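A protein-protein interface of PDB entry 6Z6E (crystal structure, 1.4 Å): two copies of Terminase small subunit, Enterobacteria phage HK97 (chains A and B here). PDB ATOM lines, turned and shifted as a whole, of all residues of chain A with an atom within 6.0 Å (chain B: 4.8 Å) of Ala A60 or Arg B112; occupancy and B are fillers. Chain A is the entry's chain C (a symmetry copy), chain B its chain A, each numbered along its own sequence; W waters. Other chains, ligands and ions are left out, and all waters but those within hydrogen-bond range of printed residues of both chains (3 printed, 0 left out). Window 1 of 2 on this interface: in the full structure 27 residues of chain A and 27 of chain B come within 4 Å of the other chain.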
ATOM      1  N   THR A  54       8.770  -6.390   2.830  1.00  0.00           N
ATOM      2  CA  THR A  54       7.452  -5.987   2.325  1.00  0.00           C
ATOM      3  C   THR A  54       6.414  -6.048   3.419  1.00  0.00           C
ATOM      4  O   THR A  54       6.632  -6.679   4.440  1.00  0.00           O
ATOM      5  CB  THR A  54       6.962  -6.877   1.185  1.00  0.00           C
ATOM      6  OG1 THR A  54       6.753  -8.212   1.715  1.00  0.00           O
ATOM      7  CG2 THR A  54       7.947  -6.971   0.081  1.00  0.00           C
ATOM      8  N   PRO A  55       5.236  -5.413   3.233  1.00  0.00           N
ATOM      9  CA  PRO A  55       4.190  -5.545   4.248  1.00  0.00           C
ATOM     10  C   PRO A  55       3.807  -7.016   4.475  1.00  0.00           C
ATOM     11  O   PRO A  55       3.559  -7.406   5.620  1.00  0.00           O
ATOM     12  CB  PRO A  55       3.045  -4.690   3.694  1.00  0.00           C
ATOM     13  CG  PRO A  55       3.763  -3.655   2.853  1.00  0.00           C
ATOM     14  CD  PRO A  55       4.894  -4.384   2.214  1.00  0.00           C
ATOM     15  N   ALA A  56       3.791  -7.795   3.409  1.00  0.00           N
ATOM     16  CA  ALA A  56       3.498  -9.255   3.550  1.00  0.00           C
ATOM     17  C   ALA A  56       4.542  -9.935   4.405  1.00  0.00           C
ATOM     18  O   ALA A  56       4.198 -10.773   5.262  1.00  0.00           O
ATOM     19  CB  ALA A  56       3.423  -9.883   2.201  1.00  0.00           C
ATOM     20  N   ASP A  57       5.810  -9.615   4.172  1.00  0.00           N
ATOM     21  CA  ASP A  57       6.890 -10.198   4.975  1.00  0.00           C
ATOM     22  C   ASP A  57       6.743  -9.837   6.433  1.00  0.00           C
ATOM     23  O   ASP A  57       7.032 -10.631   7.335  1.00  0.00           O
ATOM     24  CB  ASP A  57       8.263  -9.717   4.513  1.00  0.00           C
ATOM     25  CG  ASP A  57       8.698 -10.261   3.204  1.00  0.00           C
ATOM     26  OD1 ASP A  57       8.088 -11.214   2.637  1.00  0.00           O
ATOM     27  OD2 ASP A  57       9.713  -9.708   2.725  1.00  0.00           O
ATOM     28  N   LEU A  58       6.331  -8.597   6.720  1.00  0.00           N
ATOM     29  CA  LEU A  58       6.179  -8.183   8.108  1.00  0.00           C
ATOM     30  C   LEU A  58       5.108  -8.997   8.820  1.00  0.00           C
ATOM     31  O   LEU A  58       5.270  -9.337  10.002  1.00  0.00           O
ATOM     32  CB  LEU A  58       5.946  -6.663   8.216  1.00  0.00           C
ATOM     33  CG  LEU A  58       7.129  -5.836   7.705  1.00  0.00           C
ATOM     34  CD1 LEU A  58       6.736  -4.362   7.508  1.00  0.00           C
ATOM     35  CD2 LEU A  58       8.326  -5.882   8.639  1.00  0.00           C
ATOM     36  N   LEU A  59       4.010  -9.324   8.120  1.00  0.00           N
ATOM     37  CA  LEU A  59       2.996 -10.208   8.703  1.00  0.00           C
ATOM     38  C   LEU A  59       3.596 -11.576   9.043  1.00  0.00           C
ATOM     39  O   LEU A  59       3.389 -12.113  10.111  1.00  0.00           O
ATOM     40  CB  LEU A  59       1.843 -10.409   7.736  1.00  0.00           C
ATOM     41  CG  LEU A  59       0.963  -9.173   7.456  1.00  0.00           C
ATOM     42  CD1 LEU A  59      -0.050  -9.540   6.414  1.00  0.00           C
ATOM     43  CD2 LEU A  59       0.304  -8.661   8.713  1.00  0.00           C
ATOM     44  N   ALA A  60       4.345 -12.123   8.103  1.00  0.00           N
ATOM     45  CA  ALA A  60       4.950 -13.453   8.299  1.00  0.00           C
ATOM     46  C   ALA A  60       5.946 -13.428   9.445  1.00  0.00           C
ATOM     47  O   ALA A  60       6.038 -14.379  10.231  1.00  0.00           O
ATOM     48  CB  ALA A  60       5.620 -13.926   7.015  1.00  0.00           C
ATOM     49  N   ALA A  61       6.667 -12.333   9.582  1.00  0.00           N
ATOM     50  CA  ALA A  61       7.657 -12.204  10.640  1.00  0.00           C
ATOM     51  C   ALA A  61       7.033 -12.122  12.023  1.00  0.00           C
ATOM     52  O   ALA A  61       7.654 -12.516  13.011  1.00  0.00           O
ATOM     53  CB  ALA A  61       8.526 -10.991  10.359  1.00  0.00           C
ATOM     54  N   VAL A  62       5.795 -11.624  12.119  1.00  0.00           N
ATOM     55  CA  VAL A  62       5.116 -11.670  13.400  1.00  0.00           C
ATOM     56  C   VAL A  62       4.927 -13.108  13.862  1.00  0.00           C
ATOM     57  O   VAL A  62       5.169 -13.440  15.015  1.00  0.00           O
ATOM     58  CB  VAL A  62       3.763 -10.913  13.361  1.00  0.00           C
ATOM     59  CG1 VAL A  62       2.956 -11.207  14.615  1.00  0.00           C
ATOM     60  CG2 VAL A  62       4.012  -9.421  13.216  1.00  0.00           C
ATOM     61  N   GLU A  63       4.493 -13.977  12.951  1.00  0.00           N
ATOM     62  CA  GLU A  63       4.324 -15.369  13.312  1.00  0.00           C
ATOM     63  C   GLU A  63       5.601 -16.101  13.619  1.00  0.00           C
ATOM     64  O   GLU A  63       5.628 -16.997  14.470  1.00  0.00           O
ATOM     65  CB  GLU A  63       3.460 -16.096  12.278  1.00  0.00           C
ATOM     66  CG  GLU A  63       1.992 -15.653  12.401  1.00  0.00           C
ATOM     67  CD  GLU A  63       1.486 -15.863  13.806  1.00  0.00           C
ATOM     68  OE1 GLU A  63       1.440 -17.026  14.244  1.00  0.00           O
ATOM     69  OE2 GLU A  63       1.189 -14.876  14.573  1.00  0.00           O
ATOM     70  N   LEU A  64       6.671 -15.741  12.938  1.00  0.00           N
ATOM     71  CA  LEU A  64       7.991 -16.304  13.256  1.00  0.00           C
ATOM     72  C   LEU A  64       8.380 -15.930  14.690  1.00  0.00           C
ATOM     73  O   LEU A  64       8.738 -16.778  15.490  1.00  0.00           O
ATOM     74  CB  LEU A  64       9.022 -15.820  12.262  1.00  0.00           C
ATOM     75  CG  LEU A  64      10.493 -16.065  12.584  1.00  0.00           C
ATOM     76  CD1 LEU A  64      10.744 -17.561  12.760  1.00  0.00           C
ATOM     77  CD2 LEU A  64      11.404 -15.462  11.540  1.00  0.00           C
ATOM     78  N   ALA A  65       8.314 -14.636  14.986  1.00  0.00           N
ATOM     79  CA  ALA A  65       8.669 -14.182  16.341  1.00  0.00           C
ATOM     80  C   ALA A  65       7.777 -14.748  17.420  1.00  0.00           C
ATOM     81  O   ALA A  65       8.259 -15.171  18.486  1.00  0.00           O
ATOM     82  CB  ALA A  65       8.652 -12.651  16.380  1.00  0.00           C
ATOM     83  N   GLN A 111       9.746 -20.931   8.172  1.00  0.00           N
ATOM     84  CA  GLN A 111       9.434 -19.504   8.240  1.00  0.00           C
ATOM     85  C   GLN A 111      10.630 -18.637   7.939  1.00  0.00           C
ATOM     86  O   GLN A 111      10.511 -17.604   7.266  1.00  0.00           O
ATOM     87  CB  GLN A 111       8.856 -19.164   9.608  1.00  0.00           C
ATOM     88  CG  GLN A 111       7.487 -19.753   9.890  1.00  0.00           C
ATOM     89  CD  GLN A 111       7.042 -19.561  11.304  1.00  0.00           C
ATOM     90  OE1 GLN A 111       7.643 -20.076  12.240  1.00  0.00           O
ATOM     91  NE2 GLN A 111       5.962 -18.771  11.492  1.00  0.00           N
ATOM     92  N   ASP A 114      11.176 -18.829   4.142  1.00  0.00           N
ATOM     93  CA  ASP A 114      10.153 -18.039   3.464  1.00  0.00           C
ATOM     94  C   ASP A 114      10.499 -16.535   3.465  1.00  0.00           C
ATOM     95  O   ASP A 114      10.130 -15.840   2.513  1.00  0.00           O
ATOM     96  CB  ASP A 114       8.799 -18.306   4.128  1.00  0.00           C
ATOM     97  CG  ASP A 114       7.747 -17.267   3.780  1.00  0.00           C
ATOM     98  OD1 ASP A 114       7.044 -17.423   2.760  1.00  0.00           O
ATOM     99  OD2 ASP A 114       7.634 -16.288   4.530  1.00  0.00           O
ATOM    100  N   LEU A 115      11.183 -16.084   4.506  1.00  0.00           N
ATOM    101  CA  LEU A 115      11.565 -14.669   4.671  1.00  0.00           C
ATOM    102  C   LEU A 115      12.966 -14.363   4.162  1.00  0.00           C
ATOM    103  O   LEU A 115      13.397 -13.198   4.211  1.00  0.00           O
ATOM    104  CB  LEU A 115      11.442 -14.271   6.126  1.00  0.00           C
ATOM    105  CG  LEU A 115      10.003 -14.132   6.603  1.00  0.00           C
ATOM    106  CD1 LEU A 115       9.958 -13.989   8.117  1.00  0.00           C
ATOM    107  CD2 LEU A 115       9.307 -12.942   5.900  1.00  0.00           C
ATOM    108  N   LEU B  64      -5.557 -16.314   1.920  1.00  0.00           N
ATOM    109  CA  LEU B  64      -4.344 -15.998   2.655  1.00  0.00           C
ATOM    110  C   LEU B  64      -4.672 -15.042   3.819  1.00  0.00           C
ATOM    111  O   LEU B  64      -4.327 -15.280   4.963  1.00  0.00           O
ATOM    112  CB  LEU B  64      -3.291 -15.396   1.740  1.00  0.00           C
ATOM    113  CG  LEU B  64      -2.064 -14.767   2.380  1.00  0.00           C
ATOM    114  CD1 LEU B  64      -1.335 -15.785   3.252  1.00  0.00           C
ATOM    115  CD2 LEU B  64      -1.123 -14.207   1.339  1.00  0.00           C
ATOM    116  N   ILE B 108      -0.012 -20.878   5.125  1.00  0.00           N
ATOM    117  CA  ILE B 108       0.277 -19.502   4.722  1.00  0.00           C
ATOM    118  C   ILE B 108       1.587 -19.403   3.949  1.00  0.00           C
ATOM    119  O   ILE B 108       1.684 -18.662   2.964  1.00  0.00           O
ATOM    120  CB  ILE B 108       0.277 -18.583   5.965  1.00  0.00           C
ATOM    121  CG1 ILE B 108      -1.165 -18.348   6.457  1.00  0.00           C
ATOM    122  CG2 ILE B 108       1.027 -17.292   5.689  1.00  0.00           C
ATOM    123  CD1 ILE B 108      -1.250 -17.837   7.893  1.00  0.00           C
ATOM    124  N   LEU B 109       2.626 -20.146   4.346  1.00  0.00           N
ATOM    125  CA  LEU B 109       3.858 -20.123   3.595  1.00  0.00           C
ATOM    126  C   LEU B 109       3.633 -20.616   2.191  1.00  0.00           C
ATOM    127  O   LEU B 109       4.124 -20.016   1.225  1.00  0.00           O
ATOM    128  CB  LEU B 109       4.957 -20.951   4.288  1.00  0.00           C
ATOM    129  CG  LEU B 109       5.257 -20.631   5.733  1.00  0.00           C
ATOM    130  CD1 LEU B 109       6.446 -21.436   6.207  1.00  0.00           C
ATOM    131  CD2 LEU B 109       5.503 -19.148   5.963  1.00  0.00           C
ATOM    132  N   ALA B 110       2.856 -21.676   2.027  1.00  0.00           N
ATOM    133  CA  ALA B 110       2.533 -22.149   0.679  1.00  0.00           C
ATOM    134  C   ALA B 110       1.691 -21.155  -0.109  1.00  0.00           C
ATOM    135  O   ALA B 110       1.872 -21.013  -1.329  1.00  0.00           O
ATOM    136  CB  ALA B 110       1.839 -23.498   0.757  1.00  0.00           C
ATOM    137  N   GLN B 111       0.781 -20.480   0.571  1.00  0.00           N
ATOM    138  CA  GLN B 111      -0.071 -19.476  -0.075  1.00  0.00           C
ATOM    139  C   GLN B 111       0.724 -18.276  -0.531  1.00  0.00           C
ATOM    140  O   GLN B 111       0.473 -17.745  -1.620  1.00  0.00           O
ATOM    141  CB  GLN B 111      -1.179 -19.054   0.877  1.00  0.00           C
ATOM    142  CG  GLN B 111      -2.211 -20.145   1.184  1.00  0.00           C
ATOM    143  CD  GLN B 111      -3.177 -19.722   2.256  1.00  0.00           C
ATOM    144  OE1 GLN B 111      -2.800 -19.507   3.401  1.00  0.00           O
ATOM    145  NE2 GLN B 111      -4.462 -19.580   1.895  1.00  0.00           N
ATOM    146  N   ARG B 112       1.716 -17.880   0.258  1.00  0.00           N
ATOM    147  CA  ARG B 112       2.630 -16.797  -0.154  1.00  0.00           C
ATOM    148  C   ARG B 112       3.409 -17.150  -1.402  1.00  0.00           C
ATOM    149  O   ARG B 112       3.505 -16.365  -2.339  1.00  0.00           O
ATOM    150  CB  ARG B 112       3.550 -16.383   0.997  1.00  0.00           C
ATOM    151  CG  ARG B 112       2.876 -15.603   2.106  1.00  0.00           C
ATOM    152  CD  ARG B 112       3.691 -15.556   3.390  1.00  0.00           C
ATOM    153  NE  ARG B 112       5.104 -15.239   3.225  1.00  0.00           N
ATOM    154  CZ  ARG B 112       5.654 -14.043   3.049  1.00  0.00           C
ATOM    155  NH1 ARG B 112       4.880 -12.990   2.907  1.00  0.00           N
ATOM    156  NH2 ARG B 112       6.969 -13.934   2.969  1.00  0.00           N
ATOM    157  N   ARG B 113       3.959 -18.366  -1.439  1.00  0.00           N
ATOM    158  CA  ARG B 113       4.721 -18.800  -2.594  1.00  0.00           C
ATOM    159  C   ARG B 113       3.846 -18.890  -3.841  1.00  0.00           C
ATOM    160  O   ARG B 113       4.245 -18.472  -4.930  1.00  0.00           O
ATOM    161  CB  ARG B 113       5.369 -20.156  -2.304  1.00  0.00           C
ATOM    162  CG  ARG B 113       6.425 -20.531  -3.345  1.00  0.00           C
ATOM    163  CD  ARG B 113       7.160 -21.828  -2.979  1.00  0.00           C
ATOM    164  NE  ARG B 113       8.214 -22.137  -3.973  1.00  0.00           N
ATOM    165  CZ  ARG B 113       9.467 -21.646  -4.005  1.00  0.00           C
ATOM    166  NH1 ARG B 113      10.301 -22.056  -4.967  1.00  0.00           N
ATOM    167  NH2 ARG B 113       9.915 -20.762  -3.101  1.00  0.00           N
ATOM    168  N   ASP B 114       2.629 -19.383  -3.691  1.00  0.00           N
ATOM    169  CA  ASP B 114       1.690 -19.497  -4.810  1.00  0.00           C
ATOM    170  C   ASP B 114       1.403 -18.105  -5.438  1.00  0.00           C
ATOM    171  O   ASP B 114       1.156 -18.031  -6.637  1.00  0.00           O
ATOM    172  CB  ASP B 114       0.393 -20.162  -4.319  1.00  0.00           C
ATOM    173  CG  ASP B 114      -0.767 -19.967  -5.266  1.00  0.00           C
ATOM    174  OD1 ASP B 114      -0.945 -20.752  -6.235  1.00  0.00           O
ATOM    175  OD2 ASP B 114      -1.519 -18.995  -5.069  1.00  0.00           O
ATOM    176  N   LEU B 115       1.428 -17.068  -4.602  1.00  0.00           N
ATOM    177  CA  LEU B 115       1.151 -15.684  -5.035  1.00  0.00           C
ATOM    178  C   LEU B 115       2.402 -14.907  -5.389  1.00  0.00           C
ATOM    179  O   LEU B 115       2.294 -13.746  -5.803  1.00  0.00           O
ATOM    180  CB  LEU B 115       0.374 -14.975  -3.943  1.00  0.00           C
ATOM    181  CG  LEU B 115      -1.079 -15.416  -3.844  1.00  0.00           C
ATOM    182  CD1 LEU B 115      -1.743 -14.876  -2.575  1.00  0.00           C
ATOM    183  CD2 LEU B 115      -1.883 -15.043  -5.094  1.00  0.00           C
ATOM    184  N   GLN B 116       3.576 -15.514  -5.273  1.00  0.00           N
ATOM    185  CA  GLN B 116       4.835 -14.844  -5.498  1.00  0.00           C
ATOM    186  C   GLN B 116       4.998 -13.609  -4.614  1.00  0.00           C
ATOM    187  O   GLN B 116       5.564 -12.583  -5.041  1.00  0.00           O
ATOM    188  CB  GLN B 116       5.065 -14.552  -6.982  1.00  0.00           C
ATOM    189  CG  GLN B 116       5.146 -15.802  -7.868  1.00  0.00           C
ATOM    190  CD  GLN B 116       6.377 -16.676  -7.630  1.00  0.00           C
ATOM    191  OE1 GLN B 116       6.276 -17.875  -7.265  1.00  0.00           O
ATOM    192  NE2 GLN B 116       7.542 -16.106  -7.860  1.00  0.00           N
ATOM    193  N   ILE B 117       4.503 -13.693  -3.377  1.00  0.00           N
ATOM    194  CA  ILE B 117       4.790 -12.688  -2.363  1.00  0.00           C
ATOM    195  C   ILE B 117       5.624 -13.223  -1.202  1.00  0.00           C
ATOM    196  O   ILE B 117       5.800 -12.540  -0.193  1.00  0.00           O
ATOM    197  CB  ILE B 117       3.533 -11.955  -1.883  1.00  0.00           C
ATOM    198  CG1 ILE B 117       2.506 -12.883  -1.262  1.00  0.00           C
ATOM    199  CG2 ILE B 117       2.910 -11.186  -3.015  1.00  0.00           C
ATOM    200  CD1 ILE B 117       1.332 -12.181  -0.630  1.00  0.00           C
ATOM    201  N   HIS B 118       6.175 -14.422  -1.376  1.00  0.00           N
ATOM    202  CA  HIS B 118       7.254 -14.863  -0.484  1.00  0.00           C
ATOM    203  C   HIS B 118       8.479 -14.008  -0.738  1.00  0.00           C
ATOM    204  O   HIS B 118       8.590 -13.387  -1.785  1.00  0.00           O
ATOM    205  CB  HIS B 118       7.563 -16.363  -0.676  1.00  0.00           C
ATOM    206  CG  HIS B 118       8.007 -16.727  -2.048  1.00  0.00           C
ATOM    207  ND1 HIS B 118       7.310 -16.394  -3.199  1.00  0.00           N
ATOM    208  CD2 HIS B 118       9.092 -17.425  -2.462  1.00  0.00           C
ATOM    209  CE1 HIS B 118       7.949 -16.875  -4.253  1.00  0.00           C
ATOM    210  NE2 HIS B 118       9.038 -17.496  -3.834  1.00  0.00           N
ATOM    211  N   SER B 119       9.416 -13.983   0.183  1.00  0.00           N
ATOM    212  CA  SER B 119      10.605 -13.120   0.001  1.00  0.00           C
ATOM    213  C   SER B 119      11.461 -13.440  -1.193  1.00  0.00           C
ATOM    214  O   SER B 119      11.990 -12.510  -1.845  1.00  0.00           O
ATOM    215  CB  SER B 119      11.440 -13.081   1.258  1.00  0.00           C
ATOM    216  OG  SER B 119      10.687 -12.573   2.329  1.00  0.00           O
HETATM  217  O   HOH W   1       2.007 -12.467   3.912  1.00  0.00           O
HETATM  218  O   HOH W   2       7.267 -10.429   0.164  1.00  0.00           O
HETATM  219  O   HOH W   3       6.925 -19.420   1.164  1.00  0.00           O
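NH1 of Arg B112 sits at hydrogen-bond distance from O of Ala A56, at 3.3 Å.
OD1 of Asp A57 lies within salt-bridge range of NH2 of Arg B112 (3.0 Å).
NH2 of Arg B112 lies within salt-bridge range of OD2 of Asp A114, at 2.9 Å.
OG of Ser B119 is in hydrogen-bond range of OD1 of Asp A57 (2.9 Å).
N of Ser B119 sits at hydrogen-bond distance from O of Asp A114, at 3.1 Å.
OG of Ser B119 sits close to O of Leu A115 (3.4 Å).
The backbone NH of Ile B117 is in hydrogen-bond range of the backbone carbonyl oxygen of Arg B112 (3.0 Å).
The backbone NH (N) of His B118 sits at hydrogen-bond distance from the backbone carbonyl oxygen (O) of Arg B112 (3.4 Å).
The guanidinium group of Arg B113 sits at hydrogen-bond distance from a ring nitrogen (NE2) of His B118, 3.5 Å away.
OG1 of Thr A54 is in hydrogen-bond range of N of Asp A57, at 3.0 Å.
The backbone carbonyl oxygen (O) of Glu A63 lies close to the side-chain amide nitrogen (NE2) of Gln A111, 3.5 Å away.
N of Leu A64 lies close to NE2 of Gln A111 (3.4 Å).
Among the printed residues, pairs that only touch across the chains: Asp A57 with Ile B117 (3.9 Å), Ala A60 with Arg B112 (3.97 Å), Gln A111 with Leu B109 (3.9 Å), Asp A114 with Leu B109 (3.7 Å), Asp A114 with His B118 (3.6 Å) and Leu A115 with Arg B112 (3.9 Å).
Printed residues of chain B within 4 Å of Ala A60: Arg B112 (3.97 Å).
Arg B112 touches just these residues of chain A: Ala A56, Asp A57, Ala A60, Asp A114 and Leu A115.
Printed residues of chain A within 4 Å of Ile B117: Asp A57 (3.9 Å).
Printed residues of chain B within 4 Å of Asp A57: Arg B112 (3.0 Å), Ile B117 (3.9 Å) and Ser B119 (2.9 Å).
Of the printed residues of chain A, Leu B109 touches Gln A111 and Asp A114.
Thr A54 touches none of the printed residues of chain B.
The nearest printed residue of chain B that does not touch Ala A60 is Leu B109 (5.3 Å).
Of the 15 printed residues of chain A, 6 touch a printed residue of chain B.
Of the 13 printed residues of chain B, 5 touch a printed residue of chain A.
Among the printed residues, Asp or Glu carboxylates within 4 Å of a Lys or Arg side-chain nitrogen of the other chain: Asp A57 with Arg B112 (3.0 Å) and Asp A114 with Arg B112 (2.9 Å).
Positions printed for both chains: 64, 111, 114 and 115.
Of the 12 pairs that touch across the chains among the printed residues, none has its exchanged pair printed and touching as well.
Water W3 bridges OD1 of Asp A114 and O of Leu B109.
Water W2 lies within hydrogen-bond range of O of Ile B117 (2.6 Å), OD1 of Asp A57 (2.7 Å) and OG1 of Thr A54 (2.8 Å).
Water W1 bridges the backbone carbonyl oxygen (O) of Ala A56 (3.1 Å) and the guanidinium group (NH1) of Arg B112 (3.1 Å).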
